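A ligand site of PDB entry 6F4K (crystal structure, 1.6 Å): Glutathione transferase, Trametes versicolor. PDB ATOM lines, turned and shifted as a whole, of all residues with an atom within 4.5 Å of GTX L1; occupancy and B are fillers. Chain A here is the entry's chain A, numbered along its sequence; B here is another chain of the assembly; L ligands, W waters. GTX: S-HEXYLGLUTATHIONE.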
ATOM      1  N   PHE A  14     -29.417  -9.215  13.355  1.00  0.00           N
ATOM      2  CA  PHE A  14     -30.158 -10.238  14.078  1.00  0.00           C
ATOM      3  C   PHE A  14     -30.331  -9.913  15.570  1.00  0.00           C
ATOM      4  O   PHE A  14     -31.143 -10.583  16.213  1.00  0.00           O
ATOM      5  CB  PHE A  14     -29.478 -11.583  13.928  1.00  0.00           C
ATOM      6  CG  PHE A  14     -28.057 -11.618  14.403  1.00  0.00           C
ATOM      7  CD1 PHE A  14     -27.756 -11.692  15.774  1.00  0.00           C
ATOM      8  CD2 PHE A  14     -26.998 -11.523  13.495  1.00  0.00           C
ATOM      9  CE1 PHE A  14     -26.462 -11.698  16.209  1.00  0.00           C
ATOM     10  CE2 PHE A  14     -25.686 -11.531  13.946  1.00  0.00           C
ATOM     11  CZ  PHE A  14     -25.435 -11.585  15.307  1.00  0.00           C
ATOM     12  N   SER A  15     -29.600  -8.944  16.131  1.00  0.00           N
ATOM     13  CA  SER A  15     -29.519  -8.791  17.576  1.00  0.00           C
ATOM     14  C   SER A  15     -30.687  -7.971  18.103  1.00  0.00           C
ATOM     15  O   SER A  15     -30.719  -6.741  17.893  1.00  0.00           O
ATOM     16  CB  SER A  15     -28.222  -8.119  17.980  1.00  0.00           C
ATOM     17  OG  SER A  15     -28.243  -7.786  19.392  1.00  0.00           O
ATOM     18  N   PRO A  16     -31.687  -8.584  18.774  1.00  0.00           N
ATOM     19  CA  PRO A  16     -32.732  -7.744  19.357  1.00  0.00           C
ATOM     20  C   PRO A  16     -32.201  -6.796  20.423  1.00  0.00           C
ATOM     21  O   PRO A  16     -32.798  -5.749  20.628  1.00  0.00           O
ATOM     22  CB  PRO A  16     -33.725  -8.764  19.924  1.00  0.00           C
ATOM     23  CG  PRO A  16     -32.887 -10.009  20.151  1.00  0.00           C
ATOM     24  CD  PRO A  16     -31.842 -10.024  19.070  1.00  0.00           C
ATOM     25  N   TYR A  17     -31.121  -7.132  21.100  1.00  0.00           N
ATOM     26  CA  TYR A  17     -30.555  -6.217  22.071  1.00  0.00           C
ATOM     27  C   TYR A  17     -30.046  -4.955  21.437  1.00  0.00           C
ATOM     28  O   TYR A  17     -30.225  -3.868  21.978  1.00  0.00           O
ATOM     29  CB  TYR A  17     -29.438  -6.899  22.854  1.00  0.00           C
ATOM     30  CG  TYR A  17     -29.891  -8.051  23.716  1.00  0.00           C
ATOM     31  CD1 TYR A  17     -30.566  -7.813  24.918  1.00  0.00           C
ATOM     32  CD2 TYR A  17     -29.599  -9.363  23.368  1.00  0.00           C
ATOM     33  CE1 TYR A  17     -30.967  -8.849  25.741  1.00  0.00           C
ATOM     34  CE2 TYR A  17     -30.001 -10.415  24.203  1.00  0.00           C
ATOM     35  CZ  TYR A  17     -30.676 -10.126  25.392  1.00  0.00           C
ATOM     36  OH  TYR A  17     -31.026 -11.124  26.271  1.00  0.00           O
ATOM     37  N   ARG A  20     -32.895  -2.660  20.380  1.00  0.00           N
ATOM     38  CA  ARG A  20     -33.411  -1.812  21.451  1.00  0.00           C
ATOM     39  C   ARG A  20     -32.798  -0.425  21.365  1.00  0.00           C
ATOM     40  O   ARG A  20     -33.479   0.596  21.527  1.00  0.00           O
ATOM     41  CB  ARG A  20     -33.054  -2.401  22.831  1.00  0.00           C
ATOM     42  CG  ARG A  20     -33.639  -3.721  23.221  1.00  0.00           C
ATOM     43  CD  ARG A  20     -33.117  -4.130  24.608  1.00  0.00           C
ATOM     44  NE  ARG A  20     -34.026  -5.085  25.205  1.00  0.00           N
ATOM     45  CZ  ARG A  20     -33.772  -5.830  26.270  1.00  0.00           C
ATOM     46  NH1 ARG A  20     -32.580  -5.809  26.855  1.00  0.00           N
ATOM     47  NH2 ARG A  20     -34.737  -6.614  26.722  1.00  0.00           N
ATOM     48  N   ILE A  39     -20.462 -10.829  15.314  1.00  0.00           N
ATOM     49  CA  ILE A  39     -19.964 -11.185  16.635  1.00  0.00           C
ATOM     50  C   ILE A  39     -20.006 -12.694  16.862  1.00  0.00           C
ATOM     51  O   ILE A  39     -19.159 -13.232  17.598  1.00  0.00           O
ATOM     52  CB  ILE A  39     -20.731 -10.402  17.714  1.00  0.00           C
ATOM     53  CG1 ILE A  39     -20.185 -10.668  19.114  1.00  0.00           C
ATOM     54  CG2 ILE A  39     -22.230 -10.764  17.762  1.00  0.00           C
ATOM     55  CD1 ILE A  39     -18.735 -10.298  19.350  1.00  0.00           C
ATOM     56  N   LEU A  40     -20.971 -13.395  16.258  1.00  0.00           N
ATOM     57  CA  LEU A  40     -21.127 -14.821  16.556  1.00  0.00           C
ATOM     58  C   LEU A  40     -20.306 -15.719  15.631  1.00  0.00           C
ATOM     59  O   LEU A  40     -20.148 -16.899  15.939  1.00  0.00           O
ATOM     60  CB  LEU A  40     -22.593 -15.226  16.442  1.00  0.00           C
ATOM     61  CG  LEU A  40     -23.588 -14.479  17.348  1.00  0.00           C
ATOM     62  CD1 LEU A  40     -24.993 -15.012  17.112  1.00  0.00           C
ATOM     63  CD2 LEU A  40     -23.208 -14.555  18.808  1.00  0.00           C
ATOM     64  N   LYS A  54     -17.487  -9.041  24.963  1.00  0.00           N
ATOM     65  CA  LYS A  54     -17.548  -9.610  23.609  1.00  0.00           C
ATOM     66  C   LYS A  54     -19.001  -9.839  23.208  1.00  0.00           C
ATOM     67  O   LYS A  54     -19.351 -10.838  22.606  1.00  0.00           O
ATOM     68  CB  LYS A  54     -16.721 -10.899  23.480  1.00  0.00           C
ATOM     69  CG  LYS A  54     -15.237 -10.611  23.707  1.00  0.00           C
ATOM     70  CD  LYS A  54     -14.340 -11.861  23.572  1.00  0.00           C
ATOM     71  CE  LYS A  54     -14.491 -12.798  24.761  1.00  0.00           C
ATOM     72  NZ  LYS A  54     -13.739 -14.072  24.509  1.00  0.00           N
ATOM     73  N   LYS A  55     -19.855  -8.848  23.537  1.00  0.00           N
ATOM     74  CA  LYS A  55     -21.270  -8.883  23.188  1.00  0.00           C
ATOM     75  C   LYS A  55     -21.692  -7.630  22.425  1.00  0.00           C
ATOM     76  O   LYS A  55     -21.136  -6.539  22.607  1.00  0.00           O
ATOM     77  CB  LYS A  55     -22.142  -8.978  24.425  1.00  0.00           C
ATOM     78  CG  LYS A  55     -22.004 -10.319  25.144  1.00  0.00           C
ATOM     79  CD  LYS A  55     -22.722 -10.233  26.474  1.00  0.00           C
ATOM     80  CE  LYS A  55     -22.324 -11.369  27.385  1.00  0.00           C
ATOM     81  NZ  LYS A  55     -22.891 -12.666  26.964  1.00  0.00           N
ATOM     82  N   ILE A  56     -22.693  -7.822  21.583  1.00  0.00           N
ATOM     83  CA  ILE A  56     -23.394  -6.774  20.850  1.00  0.00           C
ATOM     84  C   ILE A  56     -24.752  -6.573  21.509  1.00  0.00           C
ATOM     85  O   ILE A  56     -25.474  -7.546  21.701  1.00  0.00           O
ATOM     86  CB  ILE A  56     -23.525  -7.177  19.378  1.00  0.00           C
ATOM     87  CG1 ILE A  56     -22.143  -7.087  18.698  1.00  0.00           C
ATOM     88  CG2 ILE A  56     -24.589  -6.412  18.630  1.00  0.00           C
ATOM     89  CD1 ILE A  56     -21.672  -5.692  18.385  1.00  0.00           C
ATOM     90  N   PRO A  57     -25.123  -5.310  21.780  1.00  0.00           N
ATOM     91  CA  PRO A  57     -24.478  -4.062  21.415  1.00  0.00           C
ATOM     92  C   PRO A  57     -23.320  -3.699  22.320  1.00  0.00           C
ATOM     93  O   PRO A  57     -23.222  -4.109  23.479  1.00  0.00           O
ATOM     94  CB  PRO A  57     -25.603  -3.029  21.571  1.00  0.00           C
ATOM     95  CG  PRO A  57     -26.421  -3.624  22.681  1.00  0.00           C
ATOM     96  CD  PRO A  57     -26.398  -5.077  22.491  1.00  0.00           C
ATOM     97  N   GLU A  80     -24.222  -3.269  27.977  1.00  0.00           N
ATOM     98  CA  GLU A  80     -25.553  -3.741  28.368  1.00  0.00           C
ATOM     99  C   GLU A  80     -26.673  -2.822  27.848  1.00  0.00           C
ATOM    100  O   GLU A  80     -26.781  -1.631  28.214  1.00  0.00           O
ATOM    101  CB  GLU A  80     -25.672  -3.948  29.894  1.00  0.00           C
ATOM    102  CG  GLU A  80     -24.717  -4.989  30.401  1.00  0.00           C
ATOM    103  CD  GLU A  80     -25.023  -6.345  29.853  1.00  0.00           C
ATOM    104  OE1 GLU A  80     -26.146  -6.845  30.136  1.00  0.00           O
ATOM    105  OE2 GLU A  80     -24.174  -6.936  29.171  1.00  0.00           O
ATOM    106  N   SER A  81     -27.552  -3.413  27.028  1.00  0.00           N
ATOM    107  CA  SER A  81     -28.550  -2.634  26.305  1.00  0.00           C
ATOM    108  C   SER A  81     -29.457  -1.795  27.209  1.00  0.00           C
ATOM    109  O   SER A  81     -29.780  -0.667  26.864  1.00  0.00           O
ATOM    110  CB  SER A  81     -29.379  -3.570  25.420  1.00  0.00           C
ATOM    111  OG  SER A  81     -30.093  -4.550  26.153  1.00  0.00           O
ATOM    112  N   GLU A 116     -37.247  -8.869  31.179  1.00  0.00           N
ATOM    113  CA  GLU A 116     -35.910  -9.422  31.282  1.00  0.00           C
ATOM    114  C   GLU A 116     -35.869 -10.619  32.230  1.00  0.00           C
ATOM    115  O   GLU A 116     -35.147 -11.594  31.980  1.00  0.00           O
ATOM    116  CB  GLU A 116     -34.953  -8.331  31.777  1.00  0.00           C
ATOM    117  CG  GLU A 116     -33.542  -8.380  31.215  1.00  0.00           C
ATOM    118  CD  GLU A 116     -33.475  -7.859  29.779  1.00  0.00           C
ATOM    119  OE1 GLU A 116     -32.390  -7.429  29.341  1.00  0.00           O
ATOM    120  OE2 GLU A 116     -34.499  -7.947  29.082  1.00  0.00           O
ATOM    121  N   PHE A 128     -34.116 -21.725  21.518  1.00  0.00           N
ATOM    122  CA  PHE A 128     -32.803 -22.353  21.447  1.00  0.00           C
ATOM    123  C   PHE A 128     -32.784 -23.794  21.946  1.00  0.00           C
ATOM    124  O   PHE A 128     -31.931 -24.573  21.500  1.00  0.00           O
ATOM    125  CB  PHE A 128     -31.773 -21.516  22.212  1.00  0.00           C
ATOM    126  CG  PHE A 128     -31.473 -20.195  21.539  1.00  0.00           C
ATOM    127  CD1 PHE A 128     -30.514 -20.099  20.553  1.00  0.00           C
ATOM    128  CD2 PHE A 128     -32.143 -19.061  21.894  1.00  0.00           C
ATOM    129  CE1 PHE A 128     -30.256 -18.902  19.926  1.00  0.00           C
ATOM    130  CE2 PHE A 128     -31.877 -17.844  21.279  1.00  0.00           C
ATOM    131  CZ  PHE A 128     -30.950 -17.775  20.306  1.00  0.00           C
ATOM    132  N   TYR A 175     -40.456 -15.142  12.866  1.00  0.00           N
ATOM    133  CA  TYR A 175     -39.696 -16.355  13.131  1.00  0.00           C
ATOM    134  C   TYR A 175     -40.608 -17.584  13.153  1.00  0.00           C
ATOM    135  O   TYR A 175     -40.228 -18.659  12.698  1.00  0.00           O
ATOM    136  CB  TYR A 175     -38.951 -16.262  14.465  1.00  0.00           C
ATOM    137  CG  TYR A 175     -37.759 -15.328  14.537  1.00  0.00           C
ATOM    138  CD1 TYR A 175     -37.428 -14.429  13.516  1.00  0.00           C
ATOM    139  CD2 TYR A 175     -36.966 -15.332  15.688  1.00  0.00           C
ATOM    140  CE1 TYR A 175     -36.321 -13.564  13.638  1.00  0.00           C
ATOM    141  CE2 TYR A 175     -35.858 -14.473  15.802  1.00  0.00           C
ATOM    142  CZ  TYR A 175     -35.556 -13.620  14.784  1.00  0.00           C
ATOM    143  OH  TYR A 175     -34.477 -12.751  14.961  1.00  0.00           O
ATOM    144  N   VAL A 233     -27.596 -17.078  12.829  1.00  0.00           N
ATOM    145  CA  VAL A 233     -27.277 -17.258  14.242  1.00  0.00           C
ATOM    146  C   VAL A 233     -27.002 -18.726  14.503  1.00  0.00           C
ATOM    147  O   VAL A 233     -27.917 -19.559  14.375  1.00  0.00           O
ATOM    148  CB  VAL A 233     -28.405 -16.739  15.143  1.00  0.00           C
ATOM    149  CG1 VAL A 233     -28.180 -17.122  16.627  1.00  0.00           C
ATOM    150  CG2 VAL A 233     -28.536 -15.224  14.996  1.00  0.00           C
ATOM    151  N   LEU A 236     -29.547 -20.813  16.642  1.00  0.00           N
ATOM    152  CA  LEU A 236     -30.880 -21.066  16.115  1.00  0.00           C
ATOM    153  C   LEU A 236     -30.919 -22.292  15.204  1.00  0.00           C
ATOM    154  O   LEU A 236     -32.026 -22.708  14.832  1.00  0.00           O
ATOM    155  CB  LEU A 236     -31.431 -19.847  15.344  1.00  0.00           C
ATOM    156  CG  LEU A 236     -31.891 -18.735  16.308  1.00  0.00           C
ATOM    157  CD1 LEU A 236     -32.282 -17.494  15.546  1.00  0.00           C
ATOM    158  CD2 LEU A 236     -33.067 -19.236  17.206  1.00  0.00           C
ATOM    159  N   ASN B 117     -27.699 -10.048  35.059  1.00  0.00           N
ATOM    160  CA  ASN B 117     -27.633 -10.881  33.880  1.00  0.00           C
ATOM    161  C   ASN B 117     -26.608 -12.002  33.884  1.00  0.00           C
ATOM    162  O   ASN B 117     -26.813 -12.981  33.253  1.00  0.00           O
ATOM    163  CB  ASN B 117     -27.421 -10.017  32.628  1.00  0.00           C
ATOM    164  CG  ASN B 117     -28.593  -9.132  32.349  1.00  0.00           C
ATOM    165  OD1 ASN B 117     -29.674  -9.367  32.783  1.00  0.00           O
ATOM    166  ND2 ASN B 117     -28.321  -8.034  31.722  1.00  0.00           N
ATOM    167  N   TYR B 118     -25.507 -11.832  34.583  1.00  0.00           N
ATOM    168  CA  TYR B 118     -24.443 -12.797  34.568  1.00  0.00           C
ATOM    169  C   TYR B 118     -23.997 -13.408  35.890  1.00  0.00           C
ATOM    170  O   TYR B 118     -23.395 -14.433  35.869  1.00  0.00           O
ATOM    171  CB  TYR B 118     -23.200 -12.161  33.882  1.00  0.00           C
ATOM    172  CG  TYR B 118     -23.518 -11.481  32.566  1.00  0.00           C
ATOM    173  CD1 TYR B 118     -24.102 -12.171  31.529  1.00  0.00           C
ATOM    174  CD2 TYR B 118     -23.282 -10.190  32.379  1.00  0.00           C
ATOM    175  CE1 TYR B 118     -24.438 -11.566  30.365  1.00  0.00           C
ATOM    176  CE2 TYR B 118     -23.607  -9.568  31.205  1.00  0.00           C
ATOM    177  CZ  TYR B 118     -24.196 -10.257  30.203  1.00  0.00           C
ATOM    178  OH  TYR B 118     -24.526  -9.626  29.059  1.00  0.00           O
HETATM  179  N1  GTX L   1     -27.425  -8.524  28.359  1.00  0.00           N
HETATM  180  CA1 GTX L   1     -26.833  -8.110  27.096  1.00  0.00           C
HETATM  181  C1  GTX L   1     -27.515  -6.818  26.674  1.00  0.00           C
HETATM  182  O11 GTX L   1     -28.606  -6.517  27.204  1.00  0.00           O
HETATM  183  O12 GTX L   1     -26.941  -6.064  25.834  1.00  0.00           O
HETATM  184  CB1 GTX L   1     -27.090  -9.189  26.044  1.00  0.00           C
HETATM  185  CG1 GTX L   1     -26.242  -8.974  24.803  1.00  0.00           C
HETATM  186  CD1 GTX L   1     -26.132 -10.266  24.001  1.00  0.00           C
HETATM  187  OE1 GTX L   1     -26.213 -11.361  24.494  1.00  0.00           O
HETATM  188  N2  GTX L   1     -25.800 -10.086  22.629  1.00  0.00           N
HETATM  189  CA2 GTX L   1     -25.568 -11.252  21.792  1.00  0.00           C
HETATM  190  C2  GTX L   1     -24.071 -11.474  21.755  1.00  0.00           C
HETATM  191  O2  GTX L   1     -23.289 -10.628  21.441  1.00  0.00           O
HETATM  192  CB2 GTX L   1     -25.960 -11.090  20.330  1.00  0.00           C
HETATM  193  SG2 GTX L   1     -27.759 -10.882  20.217  1.00  0.00           S
HETATM  194  C1S GTX L   1     -28.482 -12.238  21.183  1.00  0.00           C
HETATM  195  C2S GTX L   1     -28.241 -13.552  20.467  1.00  0.00           C
HETATM  196  C3S GTX L   1     -29.072 -13.662  19.170  1.00  0.00           C
HETATM  197  C4S GTX L   1     -30.568 -13.793  19.438  1.00  0.00           C
HETATM  198  C5S GTX L   1     -31.290 -14.067  18.127  1.00  0.00           C
HETATM  199  C6S GTX L   1     -32.756 -14.409  18.378  1.00  0.00           C
HETATM  200  N3  GTX L   1     -23.599 -12.767  22.157  1.00  0.00           N
HETATM  201  CA3 GTX L   1     -22.174 -13.067  22.141  1.00  0.00           C
HETATM  202  C3  GTX L   1     -21.836 -13.734  23.461  1.00  0.00           C
HETATM  203  O31 GTX L   1     -20.679 -14.177  23.668  1.00  0.00           O
HETATM  204  O32 GTX L   1     -22.721 -13.808  24.345  1.00  0.00           O
HETATM  205  N1  GTX L   2     -28.805 -13.662  31.275  1.00  0.00           N
HETATM  206  CA1 GTX L   2     -28.156 -13.364  29.993  1.00  0.00           C
HETATM  207  C1  GTX L   2     -28.292 -11.886  29.673  1.00  0.00           C
HETATM  208  O11 GTX L   2     -27.579 -11.409  28.768  1.00  0.00           O
HETATM  209  O12 GTX L   2     -29.104 -11.178  30.350  1.00  0.00           O
HETATM  210  CB1 GTX L   2     -28.768 -14.163  28.818  1.00  0.00           C
HETATM  211  CG1 GTX L   2     -30.282 -13.959  28.691  1.00  0.00           C
HETATM  212  CD1 GTX L   2     -30.785 -14.637  27.421  1.00  0.00           C
HETATM  213  OE1 GTX L   2     -31.198 -15.755  27.456  1.00  0.00           O
HETATM  214  N2  GTX L   2     -30.735 -13.887  26.202  1.00  0.00           N
HETATM  215  CA2 GTX L   2     -31.182 -14.493  24.951  1.00  0.00           C
HETATM  216  C2  GTX L   2     -29.918 -14.827  24.199  1.00  0.00           C
HETATM  217  O2  GTX L   2     -29.203 -13.963  23.786  1.00  0.00           O
HETATM  218  CB2 GTX L   2     -31.972 -13.495  24.140  1.00  0.00           C
HETATM  219  SG2 GTX L   2     -32.618 -14.140  22.575  1.00  0.00           S
HETATM  220  C1S GTX L   2     -34.039 -15.212  22.963  1.00  0.00           C
HETATM  221  C2S GTX L   2     -34.780 -15.583  21.669  1.00  0.00           C
HETATM  222  C3S GTX L   2     -35.826 -14.503  21.381  1.00  0.00           C
HETATM  223  C4S GTX L   2     -36.782 -14.951  20.271  1.00  0.00           C
HETATM  224  C5S GTX L   2     -37.648 -13.759  19.967  1.00  0.00           C
HETATM  225  C6S GTX L   2     -38.805 -14.248  19.091  1.00  0.00           C
HETATM  226  N3  GTX L   2     -29.613 -16.212  23.993  1.00  0.00           N
HETATM  227  CA3 GTX L   2     -28.412 -16.584  23.271  1.00  0.00           C
HETATM  228  C3  GTX L   2     -28.363 -18.109  23.275  1.00  0.00           C
HETATM  229  O31 GTX L   2     -27.626 -18.719  22.453  1.00  0.00           O
HETATM  230  O32 GTX L   2     -29.083 -18.728  24.119  1.00  0.00           O
HETATM  231  O   HOH W   1     -30.234  -9.337  28.863  1.00  0.00           O
HETATM  232  O   HOH W   2     -26.608 -13.955  23.858  1.00  0.00           O
HETATM  233  O   HOH W   3     -25.883 -12.647  26.910  1.00  0.00           O
HETATM  234  O   HOH W   4     -18.595 -13.323  22.173  1.00  0.00           O
HETATM  235  O   HOH W   5     -24.342  -5.257  25.613  1.00  0.00           O
HETATM  236  O   HOH W   6     -29.065  -4.775  29.430  1.00  0.00           O
HETATM  237  O   HOH W   7     -25.347 -15.236  21.712  1.00  0.00           O
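Merely in contact with GTX L1: Tyr 17 (3.3 Å), Asn 117 of chain B (3.5 Å), Pro 57 (3.5 Å), Lys 54 (3.6 Å), Leu 40 (3.8 Å), Ile 39 (3.8 Å), Phe 14 (3.98 Å) and Pro 16 (3.995 Å).
Within 4 Å of GTX L1: Phe 14, Ser 15, Pro 16, Tyr 17, Ile 39, Leu 40, Lys 54, Lys 55, Ile 56, Pro 57, Glu 80, Ser 81, Asn 117 of chain B and Tyr 118 of chain B.
Water W2 bridges an oxygen (O2) of GTX L2 (2.6 Å) and an oxygen (OE1) of GTX L1 (2.7 Å).
Water W4 lies within hydrogen-bond range of the backbone carbonyl oxygen (O) of Lys 54 (2.6 Å) and an oxygen (O31) of GTX L1 (2.7 Å).
Water W5 lies within hydrogen-bond range of the backbone carbonyl oxygen (O) of Pro 57 (2.7 Å), an oxygen (O12) of GTX L1 (2.7 Å) and the backbone NH (N) of Glu 80 (3.1 Å).
Water W3 lies within hydrogen-bond range of an oxygen (OE1) of GTX L1 (2.8 Å), an oxygen (O11) of GTX L2 (2.8 Å) and the side-chain amino group (NZ) of Lys 55 (3.0 Å).
Water W6 bridges O11 of GTX L1 and N of Ser 81.
Water W1 lies within hydrogen-bond range of O12 of GTX L2, OE1 of Glu 116, N1 of GTX L1 and OH of Tyr 17.
A nitrogen (N1) of GTX L1 sits at hydrogen-bond distance from an oxygen (O11) of GTX L2.
A nitrogen (N2) of GTX L2 lies within hydrogen-bond range of the side-chain hydroxyl of Tyr 17, 2.8 Å away.
An oxygen (O12) of GTX L1 sits at hydrogen-bond distance from the backbone NH (N) of Ser 81.
OG of Ser 15 sits close to SG2 of GTX L1, 3.2 Å away.
The side-chain hydroxyl (OG) of Ser 81 is in hydrogen-bond range of an oxygen (O11) of GTX L1 (2.7 Å).
The side-chain hydroxyl (OH) of Tyr 118 of chain B is in hydrogen-bond range of a nitrogen (N1) of GTX L1 (3.2 Å).
The backbone carbonyl oxygen (O) of Ile 56 is in hydrogen-bond range of a nitrogen (N2) of GTX L1, at 2.7 Å.
The side-chain carboxylate of Glu 80 lies within salt-bridge range of a nitrogen (N1) of GTX L1 (2.8 Å).
O32 of GTX L1 lies within salt-bridge range of NZ of Lys 55, at 2.9 Å.
The side-chain amide oxygen (OD1) of Asn 117 of chain B lies close to an oxygen (O12) of GTX L2, at 3.1 Å.
N of Ile 56 lies within hydrogen-bond range of O2 of GTX L1.
A nitrogen (N1) of GTX L2 sits at hydrogen-bond distance from the backbone carbonyl oxygen (O) of Asn 117 of chain B (2.9 Å).
The guanidinium group (NH1) of Arg 20 sits at hydrogen-bond distance from the side-chain hydroxyl (OG) of Ser 81 (2.9 Å).
The side-chain hydroxyl (OG) of Ser 15 sits close to the backbone NH (N) of Tyr 17 (3.4 Å).
OE1 of Glu 80 sits at hydrogen-bond distance from ND2 of Asn 117 of chain B.
The side-chain hydroxyl (OH) of Tyr 118 of chain B is in hydrogen-bond range of the side-chain carboxylate (OE2) of Glu 80.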
